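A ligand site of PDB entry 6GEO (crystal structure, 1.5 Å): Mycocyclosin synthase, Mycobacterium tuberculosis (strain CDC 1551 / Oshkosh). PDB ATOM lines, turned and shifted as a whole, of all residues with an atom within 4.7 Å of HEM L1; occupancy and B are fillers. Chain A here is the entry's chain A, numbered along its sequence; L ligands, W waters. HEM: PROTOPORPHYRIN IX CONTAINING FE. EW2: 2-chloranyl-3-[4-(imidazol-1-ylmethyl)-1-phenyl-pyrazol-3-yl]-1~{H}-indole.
SG of Cys 345 binds FE of HEM L1, at 2.3 Å. O1A of HEM L1 is in salt-bridge range of NH2 of Arg 286, at 2.7 Å. An oxygen (O1D) of HEM L1 lies within hydrogen-bond range of a ring nitrogen (ND1) of His 343 (2.8 Å).
Water W2 lies within hydrogen-bond range of O2D of HEM L1 (2.7 Å), N of Met 86 (3.0 Å) and SD of Met 62 (3.6 Å). Water W5 lies within hydrogen-bond range of O1D of HEM L1 and O of Phe 344. Water W6 bridges O2D of HEM L1 (3.0 Å) and SD of Met 62 (3.5 Å). Water W3 bridges O of Gln 342 and O1D of HEM L1.
The side-chain sulfur (SD) of Met 62 sits close to an oxygen (O2D) of HEM L1 (3.4 Å). CG of Met 86 touches O1D of HEM L1 (3.2 Å). His 146 touches HEM L1. Phe 230 touches HEM L1 (CZ to CMD, 3.5 Å). Gly 234 touches HEM L1 (CA to C2C, 3.5 Å). Ser 237 touches HEM L1 (CB to C4B, 3.4 Å). CG2 of Thr 238 touches CMC of HEM L1 (3.7 Å). CB of Phe 241 touches CBB of HEM L1, at 3.7 Å. Phe 280 touches HEM L1 (CE1 to CHB, 3.5 Å). Leu 284 touches HEM L1 (CD1 to CGA, 3.7 Å). Leu 309 touches HEM L1. O of Ala 337 touches CMA of HEM L1, at 3.3 Å. Phe 338 touches HEM L1 (C to CMA, 3.6 Å). Gly 339 touches HEM L1. Pro 346 touches HEM L1. Gly 347 touches HEM L1. Leu 350 touches HEM L1. Hydrophobic or aromatic side chains that line HEM L1: Met 62, Met 86, His 146, Phe 230, Phe 241, Phe 280, Leu 284, Leu 309, Phe 338, His 343, Pro 346 and Leu 350. Of the 28 residues printed, 20 come within 4 Å of HEM L1. The nearest printed residue that does not touch HEM L1 is Leu 274 (4.03 Å).
The backbone NH of Cys 345 sits at hydrogen-bond distance from the backbone carbonyl oxygen of Phe 338, 2.9 Å away. SG of Cys 345 sits close to N of Gly 347 (3.3 Å). A ring nitrogen (ND1) of His 343 is in hydrogen-bond range of the side-chain sulfur of Met 62 (3.4 Å). O of Ala 233 sits at hydrogen-bond distance from OG of Ser 237 (2.7 Å). O of Gly 234 is in hydrogen-bond range of OG1 of Thr 238 (2.7 Å).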
ATOM      1  N   MET A  62     -16.253  -2.174  32.631  1.00  0.00           N
ATOM      2  CA  MET A  62     -16.188  -3.613  32.483  1.00  0.00           C
ATOM      3  C   MET A  62     -14.831  -4.135  32.875  1.00  0.00           C
ATOM      4  O   MET A  62     -14.707  -5.094  33.652  1.00  0.00           O
ATOM      5  CB  MET A  62     -16.542  -4.057  31.031  1.00  0.00           C
ATOM      6  CG  MET A  62     -16.231  -5.531  30.695  1.00  0.00           C
ATOM      7  SD  MET A  62     -16.723  -5.859  29.005  1.00  0.00           S
ATOM      8  CE  MET A  62     -18.513  -5.976  29.187  1.00  0.00           C
ATOM      9  N   MET A  86     -13.002  -7.341  23.955  1.00  0.00           N
ATOM     10  CA  MET A  86     -13.261  -6.414  22.862  1.00  0.00           C
ATOM     11  C   MET A  86     -12.256  -5.272  22.816  1.00  0.00           C
ATOM     12  O   MET A  86     -11.835  -4.831  21.739  1.00  0.00           O
ATOM     13  CB  MET A  86     -14.691  -5.871  22.907  1.00  0.00           C
ATOM     14  CG  MET A  86     -15.765  -6.820  22.410  1.00  0.00           C
ATOM     15  SD  MET A  86     -15.598  -7.444  20.722  1.00  0.00           S
ATOM     16  CE  MET A  86     -15.221  -5.967  19.834  1.00  0.00           C
ATOM     17  N   ILE A 102     -18.917 -11.573  11.543  1.00  0.00           N
ATOM     18  CA  ILE A 102     -19.987 -12.191  12.342  1.00  0.00           C
ATOM     19  C   ILE A 102     -21.341 -11.540  12.051  1.00  0.00           C
ATOM     20  O   ILE A 102     -22.298 -11.728  12.802  1.00  0.00           O
ATOM     21  CB  ILE A 102     -19.656 -12.180  13.851  1.00  0.00           C
ATOM     22  CG1 ILE A 102     -19.645 -10.781  14.426  1.00  0.00           C
ATOM     23  CG2 ILE A 102     -18.349 -12.886  14.095  1.00  0.00           C
ATOM     24  CD1 ILE A 102     -19.505 -10.794  15.941  1.00  0.00           C
ATOM     25  N   HIS A 146     -22.452 -21.278  14.228  1.00  0.00           N
ATOM     26  CA  HIS A 146     -21.173 -20.675  14.599  1.00  0.00           C
ATOM     27  C   HIS A 146     -20.009 -21.423  14.019  1.00  0.00           C
ATOM     28  O   HIS A 146     -18.971 -20.787  13.769  1.00  0.00           O
ATOM     29  CB  HIS A 146     -21.108 -20.550  16.123  1.00  0.00           C
ATOM     30  CG  HIS A 146     -21.911 -19.405  16.629  1.00  0.00           C
ATOM     31  ND1 HIS A 146     -23.287 -19.505  16.771  1.00  0.00           N
ATOM     32  CD2 HIS A 146     -21.602 -18.124  16.882  1.00  0.00           C
ATOM     33  CE1 HIS A 146     -23.765 -18.318  17.151  1.00  0.00           C
ATOM     34  NE2 HIS A 146     -22.765 -17.453  17.196  1.00  0.00           N
ATOM     35  N   PHE A 230     -15.673 -15.987  20.781  1.00  0.00           N
ATOM     36  CA  PHE A 230     -16.828 -15.685  19.955  1.00  0.00           C
ATOM     37  C   PHE A 230     -17.647 -16.924  19.680  1.00  0.00           C
ATOM     38  O   PHE A 230     -18.888 -16.855  19.673  1.00  0.00           O
ATOM     39  CB  PHE A 230     -16.396 -14.980  18.630  1.00  0.00           C
ATOM     40  CG  PHE A 230     -16.181 -13.492  18.801  1.00  0.00           C
ATOM     41  CD1 PHE A 230     -15.268 -12.990  19.702  1.00  0.00           C
ATOM     42  CD2 PHE A 230     -16.984 -12.591  18.097  1.00  0.00           C
ATOM     43  CE1 PHE A 230     -15.116 -11.620  19.892  1.00  0.00           C
ATOM     44  CE2 PHE A 230     -16.843 -11.263  18.283  1.00  0.00           C
ATOM     45  CZ  PHE A 230     -15.938 -10.763  19.152  1.00  0.00           C
ATOM     46  N   ALA A 233     -19.495 -17.419  23.335  1.00  0.00           N
ATOM     47  CA  ALA A 233     -20.499 -16.401  23.595  1.00  0.00           C
ATOM     48  C   ALA A 233     -21.656 -16.482  22.605  1.00  0.00           C
ATOM     49  O   ALA A 233     -22.817 -16.415  22.974  1.00  0.00           O
ATOM     50  CB  ALA A 233     -19.888 -15.014  23.555  1.00  0.00           C
ATOM     51  N   GLY A 234     -21.341 -16.644  21.307  1.00  0.00           N
ATOM     52  CA  GLY A 234     -22.414 -16.693  20.349  1.00  0.00           C
ATOM     53  C   GLY A 234     -23.293 -17.911  20.500  1.00  0.00           C
ATOM     54  O   GLY A 234     -24.511 -17.817  20.466  1.00  0.00           O
ATOM     55  N   SER A 237     -25.349 -17.777  23.729  1.00  0.00           N
ATOM     56  CA  SER A 237     -26.313 -16.700  23.748  1.00  0.00           C
ATOM     57  C   SER A 237     -27.467 -16.980  22.791  1.00  0.00           C
ATOM     58  O   SER A 237     -28.636 -16.812  23.144  1.00  0.00           O
ATOM     59  CB  SER A 237     -25.679 -15.363  23.407  1.00  0.00           C
ATOM     60  OG  SER A 237     -24.667 -14.984  24.323  1.00  0.00           O
ATOM     61  N   THR A 238     -27.158 -17.416  21.573  1.00  0.00           N
ATOM     62  CA  THR A 238     -28.207 -17.699  20.590  1.00  0.00           C
ATOM     63  C   THR A 238     -28.980 -18.968  20.933  1.00  0.00           C
ATOM     64  O   THR A 238     -30.215 -19.000  20.800  1.00  0.00           O
ATOM     65  CB  THR A 238     -27.634 -17.818  19.164  1.00  0.00           C
ATOM     66  OG1 THR A 238     -26.656 -18.830  19.103  1.00  0.00           O
ATOM     67  CG2 THR A 238     -27.082 -16.457  18.670  1.00  0.00           C
ATOM     68  N   PHE A 241     -31.167 -17.978  24.015  1.00  0.00           N
ATOM     69  CA  PHE A 241     -32.228 -17.040  23.673  1.00  0.00           C
ATOM     70  C   PHE A 241     -33.281 -17.733  22.827  1.00  0.00           C
ATOM     71  O   PHE A 241     -34.479 -17.631  23.128  1.00  0.00           O
ATOM     72  CB  PHE A 241     -31.701 -15.813  22.896  1.00  0.00           C
ATOM     73  CG  PHE A 241     -32.828 -15.061  22.310  1.00  0.00           C
ATOM     74  CD1 PHE A 241     -33.746 -14.442  23.153  1.00  0.00           C
ATOM     75  CD2 PHE A 241     -33.060 -15.021  20.947  1.00  0.00           C
ATOM     76  CE1 PHE A 241     -34.873 -13.805  22.631  1.00  0.00           C
ATOM     77  CE2 PHE A 241     -34.176 -14.366  20.453  1.00  0.00           C
ATOM     78  CZ  PHE A 241     -35.079 -13.795  21.285  1.00  0.00           C
ATOM     79  N   LEU A 274     -37.006 -10.763  22.136  1.00  0.00           N
ATOM     80  CA  LEU A 274     -35.752 -10.244  22.716  1.00  0.00           C
ATOM     81  C   LEU A 274     -36.062  -9.356  23.887  1.00  0.00           C
ATOM     82  O   LEU A 274     -35.476  -9.495  24.981  1.00  0.00           O
ATOM     83  CB  LEU A 274     -34.961  -9.475  21.645  1.00  0.00           C
ATOM     84  CG  LEU A 274     -34.208 -10.367  20.681  1.00  0.00           C
ATOM     85  CD1 LEU A 274     -33.813  -9.575  19.394  1.00  0.00           C
ATOM     86  CD2 LEU A 274     -32.936 -10.973  21.344  1.00  0.00           C
ATOM     87  N   SER A 279     -33.019 -14.610  29.351  1.00  0.00           N
ATOM     88  CA  SER A 279     -31.867 -15.511  29.178  1.00  0.00           C
ATOM     89  C   SER A 279     -30.663 -15.116  29.999  1.00  0.00           C
ATOM     90  O   SER A 279     -29.936 -16.017  30.445  1.00  0.00           O
ATOM     91  CB  SER A 279     -31.431 -15.642  27.691  1.00  0.00           C
ATOM     92  OG  SER A 279     -30.747 -14.504  27.172  1.00  0.00           O
ATOM     93  N   PHE A 280     -30.416 -13.847  30.256  1.00  0.00           N
ATOM     94  CA  PHE A 280     -29.304 -13.480  31.133  1.00  0.00           C
ATOM     95  C   PHE A 280     -29.695 -13.704  32.589  1.00  0.00           C
ATOM     96  O   PHE A 280     -30.618 -13.100  33.104  1.00  0.00           O
ATOM     97  CB  PHE A 280     -28.819 -12.068  30.905  1.00  0.00           C
ATOM     98  CG  PHE A 280     -27.808 -11.942  29.812  1.00  0.00           C
ATOM     99  CD1 PHE A 280     -28.150 -12.257  28.525  1.00  0.00           C
ATOM    100  CD2 PHE A 280     -26.495 -11.581  30.078  1.00  0.00           C
ATOM    101  CE1 PHE A 280     -27.195 -12.162  27.513  1.00  0.00           C
ATOM    102  CE2 PHE A 280     -25.565 -11.460  29.058  1.00  0.00           C
ATOM    103  CZ  PHE A 280     -25.922 -11.770  27.797  1.00  0.00           C
ATOM    104  N   LEU A 284     -25.711  -7.387  34.335  1.00  0.00           N
ATOM    105  CA  LEU A 284     -24.401  -7.110  33.719  1.00  0.00           C
ATOM    106  C   LEU A 284     -23.471  -6.396  34.719  1.00  0.00           C
ATOM    107  O   LEU A 284     -23.864  -5.369  35.286  1.00  0.00           O
ATOM    108  CB  LEU A 284     -24.517  -6.240  32.467  1.00  0.00           C
ATOM    109  CG  LEU A 284     -25.447  -6.795  31.387  1.00  0.00           C
ATOM    110  CD1 LEU A 284     -25.469  -5.833  30.211  1.00  0.00           C
ATOM    111  CD2 LEU A 284     -25.016  -8.160  30.904  1.00  0.00           C
ATOM    112  N   ARG A 286     -20.389  -4.174  36.351  1.00  0.00           N
ATOM    113  CA  ARG A 286     -19.508  -3.034  36.128  1.00  0.00           C
ATOM    114  C   ARG A 286     -18.910  -2.630  37.456  1.00  0.00           C
ATOM    115  O   ARG A 286     -19.532  -2.799  38.501  1.00  0.00           O
ATOM    116  CB  ARG A 286     -20.267  -1.848  35.557  1.00  0.00           C
ATOM    117  CG  ARG A 286     -20.908  -2.064  34.197  1.00  0.00           C
ATOM    118  CD  ARG A 286     -19.932  -2.190  33.101  1.00  0.00           C
ATOM    119  NE  ARG A 286     -20.535  -2.178  31.746  1.00  0.00           N
ATOM    120  CZ  ARG A 286     -20.923  -3.243  31.079  1.00  0.00           C
ATOM    121  NH1 ARG A 286     -20.837  -4.461  31.591  1.00  0.00           N
ATOM    122  NH2 ARG A 286     -21.415  -3.094  29.835  1.00  0.00           N
ATOM    123  N   LEU A 309     -31.091  -6.562  33.168  1.00  0.00           N
ATOM    124  CA  LEU A 309     -31.672  -6.319  31.822  1.00  0.00           C
ATOM    125  C   LEU A 309     -33.188  -6.397  31.851  1.00  0.00           C
ATOM    126  O   LEU A 309     -33.863  -5.534  31.255  1.00  0.00           O
ATOM    127  CB  LEU A 309     -31.109  -7.274  30.817  1.00  0.00           C
ATOM    128  CG  LEU A 309     -29.613  -7.135  30.598  1.00  0.00           C
ATOM    129  CD1 LEU A 309     -29.107  -8.085  29.538  1.00  0.00           C
ATOM    130  CD2 LEU A 309     -29.179  -5.684  30.305  1.00  0.00           C
ATOM    131  N   LEU A 336     -32.835  -3.429  25.990  1.00  0.00           N
ATOM    132  CA  LEU A 336     -31.431  -3.636  26.397  1.00  0.00           C
ATOM    133  C   LEU A 336     -31.034  -5.104  26.267  1.00  0.00           C
ATOM    134  O   LEU A 336     -30.043  -5.516  26.859  1.00  0.00           O
ATOM    135  CB  LEU A 336     -31.182  -3.163  27.820  1.00  0.00           C
ATOM    136  CG  LEU A 336     -31.549  -1.727  28.117  1.00  0.00           C
ATOM    137  CD1 LEU A 336     -30.939  -1.305  29.472  1.00  0.00           C
ATOM    138  CD2 LEU A 336     -31.113  -0.788  27.073  1.00  0.00           C
ATOM    139  N   ALA A 337     -31.741  -5.919  25.468  1.00  0.00           N
ATOM    140  CA  ALA A 337     -31.363  -7.331  25.351  1.00  0.00           C
ATOM    141  C   ALA A 337     -29.946  -7.545  24.861  1.00  0.00           C
ATOM    142  O   ALA A 337     -29.326  -8.568  25.168  1.00  0.00           O
ATOM    143  CB  ALA A 337     -32.332  -8.089  24.427  1.00  0.00           C
ATOM    144  N   PHE A 338     -29.405  -6.617  24.056  1.00  0.00           N
ATOM    145  CA  PHE A 338     -28.024  -6.677  23.563  1.00  0.00           C
ATOM    146  C   PHE A 338     -27.106  -5.720  24.311  1.00  0.00           C
ATOM    147  O   PHE A 338     -26.003  -5.412  23.832  1.00  0.00           O
ATOM    148  CB  PHE A 338     -28.026  -6.371  22.063  1.00  0.00           C
ATOM    149  CG  PHE A 338     -28.733  -7.414  21.222  1.00  0.00           C
ATOM    150  CD1 PHE A 338     -28.273  -8.714  21.179  1.00  0.00           C
ATOM    151  CD2 PHE A 338     -29.811  -7.090  20.416  1.00  0.00           C
ATOM    152  CE1 PHE A 338     -28.887  -9.664  20.414  1.00  0.00           C
ATOM    153  CE2 PHE A 338     -30.424  -8.038  19.619  1.00  0.00           C
ATOM    154  CZ  PHE A 338     -29.972  -9.325  19.592  1.00  0.00           C
ATOM    155  N   GLY A 339     -27.541  -5.211  25.455  1.00  0.00           N
ATOM    156  CA  GLY A 339     -26.745  -4.229  26.132  1.00  0.00           C
ATOM    157  C   GLY A 339     -26.953  -2.857  25.510  1.00  0.00           C
ATOM    158  O   GLY A 339     -27.958  -2.599  24.831  1.00  0.00           O
ATOM    159  N   GLN A 342     -20.715   1.207  25.199  1.00  0.00           N
ATOM    160  CA  GLN A 342     -19.421   0.736  24.716  1.00  0.00           C
ATOM    161  C   GLN A 342     -19.405  -0.744  24.408  1.00  0.00           C
ATOM    162  O   GLN A 342     -18.719  -1.174  23.485  1.00  0.00           O
ATOM    163  CB  GLN A 342     -18.349   1.053  25.762  1.00  0.00           C
ATOM    164  CG  GLN A 342     -16.946   0.593  25.418  1.00  0.00           C
ATOM    165  CD  GLN A 342     -16.309   1.437  24.343  1.00  0.00           C
ATOM    166  OE1 GLN A 342     -16.793   2.550  24.008  1.00  0.00           O
ATOM    167  NE2 GLN A 342     -15.208   0.932  23.777  1.00  0.00           N
ATOM    168  N   HIS A 343     -20.158  -1.545  25.160  1.00  0.00           N
ATOM    169  CA  HIS A 343     -20.058  -2.998  25.087  1.00  0.00           C
ATOM    170  C   HIS A 343     -21.278  -3.634  24.426  1.00  0.00           C
ATOM    171  O   HIS A 343     -21.534  -4.829  24.596  1.00  0.00           O
ATOM    172  CB  HIS A 343     -19.785  -3.562  26.486  1.00  0.00           C
ATOM    173  CG  HIS A 343     -18.482  -3.111  27.034  1.00  0.00           C
ATOM    174  ND1 HIS A 343     -17.305  -3.572  26.517  1.00  0.00           N
ATOM    175  CD2 HIS A 343     -18.172  -2.184  27.962  1.00  0.00           C
ATOM    176  CE1 HIS A 343     -16.304  -2.969  27.142  1.00  0.00           C
ATOM    177  NE2 HIS A 343     -16.801  -2.120  28.001  1.00  0.00           N
ATOM    178  N   PHE A 344     -22.049  -2.827  23.671  1.00  0.00           N
ATOM    179  CA  PHE A 344     -23.191  -3.344  22.925  1.00  0.00           C
ATOM    180  C   PHE A 344     -22.781  -4.589  22.124  1.00  0.00           C
ATOM    181  O   PHE A 344     -21.737  -4.642  21.497  1.00  0.00           O
ATOM    182  CB  PHE A 344     -23.712  -2.259  21.949  1.00  0.00           C
ATOM    183  CG  PHE A 344     -24.940  -2.656  21.185  1.00  0.00           C
ATOM    184  CD1 PHE A 344     -26.164  -2.537  21.743  1.00  0.00           C
ATOM    185  CD2 PHE A 344     -24.835  -3.197  19.946  1.00  0.00           C
ATOM    186  CE1 PHE A 344     -27.292  -2.938  21.060  1.00  0.00           C
ATOM    187  CE2 PHE A 344     -25.983  -3.622  19.235  1.00  0.00           C
ATOM    188  CZ  PHE A 344     -27.192  -3.488  19.807  1.00  0.00           C
ATOM    189  N   CYS A 345     -23.664  -5.617  22.152  1.00  0.00           N
ATOM    190  CA  CYS A 345     -23.338  -6.898  21.543  1.00  0.00           C
ATOM    191  C   CYS A 345     -22.916  -6.771  20.068  1.00  0.00           C
ATOM    192  O   CYS A 345     -23.730  -6.327  19.270  1.00  0.00           O
ATOM    193  CB  CYS A 345     -24.548  -7.830  21.631  1.00  0.00           C
ATOM    194  SG  CYS A 345     -24.231  -9.465  20.922  1.00  0.00           S
ATOM    195  N   PRO A 346     -21.732  -7.243  19.696  1.00  0.00           N
ATOM    196  CA  PRO A 346     -21.329  -7.196  18.291  1.00  0.00           C
ATOM    197  C   PRO A 346     -22.005  -8.253  17.440  1.00  0.00           C
ATOM    198  O   PRO A 346     -21.875  -8.223  16.195  1.00  0.00           O
ATOM    199  CB  PRO A 346     -19.836  -7.401  18.342  1.00  0.00           C
ATOM    200  CG  PRO A 346     -19.648  -8.271  19.519  1.00  0.00           C
ATOM    201  CD  PRO A 346     -20.659  -7.774  20.544  1.00  0.00           C
ATOM    202  N   GLY A 347     -22.689  -9.210  18.049  1.00  0.00           N
ATOM    203  CA  GLY A 347     -23.392 -10.279  17.380  1.00  0.00           C
ATOM    204  C   GLY A 347     -24.869 -10.047  17.208  1.00  0.00           C
ATOM    205  O   GLY A 347     -25.599 -11.000  16.877  1.00  0.00           O
ATOM    206  N   LEU A 350     -26.601 -11.162  13.909  1.00  0.00           N
ATOM    207  CA  LEU A 350     -26.555 -12.613  13.791  1.00  0.00           C
ATOM    208  C   LEU A 350     -27.547 -13.267  14.738  1.00  0.00           C
ATOM    209  O   LEU A 350     -28.185 -14.263  14.400  1.00  0.00           O
ATOM    210  CB  LEU A 350     -25.144 -13.091  14.042  1.00  0.00           C
ATOM    211  CG  LEU A 350     -24.859 -14.523  13.747  1.00  0.00           C
ATOM    212  CD1 LEU A 350     -25.075 -14.858  12.252  1.00  0.00           C
ATOM    213  CD2 LEU A 350     -23.478 -14.917  14.130  1.00  0.00           C
ATOM    214  N   GLY A 351     -27.633 -12.762  15.972  1.00  0.00           N
ATOM    215  CA  GLY A 351     -28.542 -13.340  16.937  1.00  0.00           C
ATOM    216  C   GLY A 351     -29.989 -13.178  16.519  1.00  0.00           C
ATOM    217  O   GLY A 351     -30.803 -14.108  16.606  1.00  0.00           O
HETATM  218  CHA HEM L   1     -21.964  -8.748  24.515  1.00  0.00           C
HETATM  219  CHB HEM L   1     -26.487 -10.460  24.489  1.00  0.00           C
HETATM  220  CHC HEM L   1     -25.463 -13.039  20.553  1.00  0.00           C
HETATM  221  CHD HEM L   1     -20.828 -11.973  21.054  1.00  0.00           C
HETATM  222  C1A HEM L   1     -23.314  -8.888  24.778  1.00  0.00           C
HETATM  223  C2A HEM L   1     -24.042  -8.155  25.798  1.00  0.00           C
HETATM  224  C3A HEM L   1     -25.285  -8.700  25.809  1.00  0.00           C
HETATM  225  C4A HEM L   1     -25.368  -9.720  24.794  1.00  0.00           C
HETATM  226  CMA HEM L   1     -26.411  -8.274  26.738  1.00  0.00           C
HETATM  227  CAA HEM L   1     -23.450  -7.028  26.665  1.00  0.00           C
HETATM  228  CBA HEM L   1     -22.592  -7.514  27.829  1.00  0.00           C
HETATM  229  CGA HEM L   1     -22.179  -6.347  28.682  1.00  0.00           C
HETATM  230  O1A HEM L   1     -22.376  -5.155  28.337  1.00  0.00           O
HETATM  231  O2A HEM L   1     -21.623  -6.628  29.835  1.00  0.00           O
HETATM  232  C1B HEM L   1     -26.600 -11.354  23.406  1.00  0.00           C
HETATM  233  C2B HEM L   1     -27.853 -11.960  23.019  1.00  0.00           C
HETATM  234  C3B HEM L   1     -27.547 -12.683  21.942  1.00  0.00           C
HETATM  235  C4B HEM L   1     -26.132 -12.530  21.621  1.00  0.00           C
HETATM  236  CMB HEM L   1     -29.192 -11.834  23.746  1.00  0.00           C
HETATM  237  CAB HEM L   1     -28.410 -13.554  21.047  1.00  0.00           C
HETATM  238  CBB HEM L   1     -29.732 -13.386  20.937  1.00  0.00           C
HETATM  239  C1C HEM L   1     -24.133 -12.948  20.317  1.00  0.00           C
HETATM  240  C2C HEM L   1     -23.439 -13.542  19.192  1.00  0.00           C
HETATM  241  C3C HEM L   1     -22.114 -13.238  19.381  1.00  0.00           C
HETATM  242  C4C HEM L   1     -22.001 -12.461  20.560  1.00  0.00           C
HETATM  243  CMC HEM L   1     -24.092 -14.309  18.027  1.00  0.00           C
HETATM  244  CAC HEM L   1     -20.924 -13.640  18.507  1.00  0.00           C
HETATM  245  CBC HEM L   1     -20.959 -14.497  17.492  1.00  0.00           C
HETATM  246  C1D HEM L   1     -20.716 -11.028  22.081  1.00  0.00           C
HETATM  247  C2D HEM L   1     -19.485 -10.388  22.527  1.00  0.00           C
HETATM  248  C3D HEM L   1     -19.800  -9.487  23.499  1.00  0.00           C
HETATM  249  C4D HEM L   1     -21.222  -9.544  23.652  1.00  0.00           C
HETATM  250  CMD HEM L   1     -18.120 -10.790  21.951  1.00  0.00           C
HETATM  251  CAD HEM L   1     -18.851  -8.576  24.333  1.00  0.00           C
HETATM  252  CBD HEM L   1     -18.849  -7.169  23.868  1.00  0.00           C
HETATM  253  CGD HEM L   1     -17.957  -6.267  24.760  1.00  0.00           C
HETATM  254  O1D HEM L   1     -17.760  -5.179  24.289  1.00  0.00           O
HETATM  255  O2D HEM L   1     -17.568  -6.718  25.862  1.00  0.00           O
HETATM  256  NA  HEM L   1     -24.145  -9.854  24.187  1.00  0.00           N
HETATM  257  NB  HEM L   1     -25.556 -11.702  22.583  1.00  0.00           N
HETATM  258  NC  HEM L   1     -23.251 -12.252  21.134  1.00  0.00           N
HETATM  259  ND  HEM L   1     -21.753 -10.508  22.774  1.00  0.00           N
HETATM  260 FE   HEM L   1     -23.703 -10.960  22.572  1.00  0.00          FE
HETATM  261  C10 EW2 L   2     -17.994 -15.193  30.633  1.00  0.00           C
HETATM  262  C13 EW2 L   2     -16.145 -15.685  33.649  1.00  0.00           C
HETATM  263  C15 EW2 L   2     -17.843 -14.546  33.050  1.00  0.00           C
HETATM  264  C17 EW2 L   2     -16.335 -13.662  28.221  1.00  0.00           C
HETATM  265  C21 EW2 L   2     -16.410 -13.095  26.925  1.00  0.00           C
HETATM  266  C22 EW2 L   2     -16.201 -11.744  27.089  1.00  0.00           C
HETATM  267  C24 EW2 L   2     -16.660 -13.628  25.662  1.00  0.00           C
HETATM  268  C26 EW2 L   2     -16.444 -11.416  24.694  1.00  0.00           C
HETATM  269  C02 EW2 L   2     -15.881 -18.445  27.415  1.00  0.00           C
HETATM  270  C03 EW2 L   2     -16.115 -18.484  26.033  1.00  0.00           C
HETATM  271  C04 EW2 L   2     -15.782 -19.618  25.327  1.00  0.00           C
HETATM  272  C05 EW2 L   2     -15.241 -20.748  25.992  1.00  0.00           C
HETATM  273  C06 EW2 L   2     -15.010 -20.682  27.363  1.00  0.00           C
HETATM  274  C07 EW2 L   2     -15.383 -19.537  28.079  1.00  0.00           C
HETATM  275  C08 EW2 L   2     -17.036 -17.178  29.232  1.00  0.00           C
HETATM  276  C09 EW2 L   2     -17.200 -15.845  29.516  1.00  0.00           C
HETATM  277  C12 EW2 L   2     -16.363 -15.953  32.331  1.00  0.00           C
HETATM  278  C16 EW2 L   2     -16.505 -15.155  28.472  1.00  0.00           C
HETATM  279  C18 EW2 L   2     -16.070 -12.599  29.066  1.00  0.00           C
HETATM  280  C23 EW2 L   2     -16.200 -10.913  25.935  1.00  0.00           C
HETATM  281  C25 EW2 L   2     -16.673 -12.793  24.534  1.00  0.00           C
HETATM  282  N01 EW2 L   2     -16.282 -17.268  28.104  1.00  0.00           N
HETATM  283  N11 EW2 L   2     -17.410 -15.252  31.984  1.00  0.00           N
HETATM  284  N14 EW2 L   2     -17.084 -14.856  34.110  1.00  0.00           N
HETATM  285  N19 EW2 L   2     -15.982 -11.477  28.385  1.00  0.00           N
HETATM  286  N27 EW2 L   2     -15.982 -16.034  27.630  1.00  0.00           N
HETATM  287 CL2  EW2 L   2     -15.774 -12.631  30.789  1.00  0.00          CL
HETATM  288  O   HOH W   1     -23.207 -12.634  24.085  1.00  0.00           O
HETATM  289  O   HOH W   2     -14.950  -7.323  26.264  1.00  0.00           O
HETATM  290  O   HOH W   3     -16.149  -2.631  23.199  1.00  0.00           O
HETATM  291  O   HOH W   4     -20.817  -9.001  30.742  1.00  0.00           O
HETATM  292  O   HOH W   5     -18.877  -4.504  21.811  1.00  0.00           O
HETATM  293  O   HOH W   6     -18.387  -8.719  27.961  1.00  0.00           O
HETATM  294  O   HOH W   7     -23.636  -3.255  26.927  1.00  0.00           O
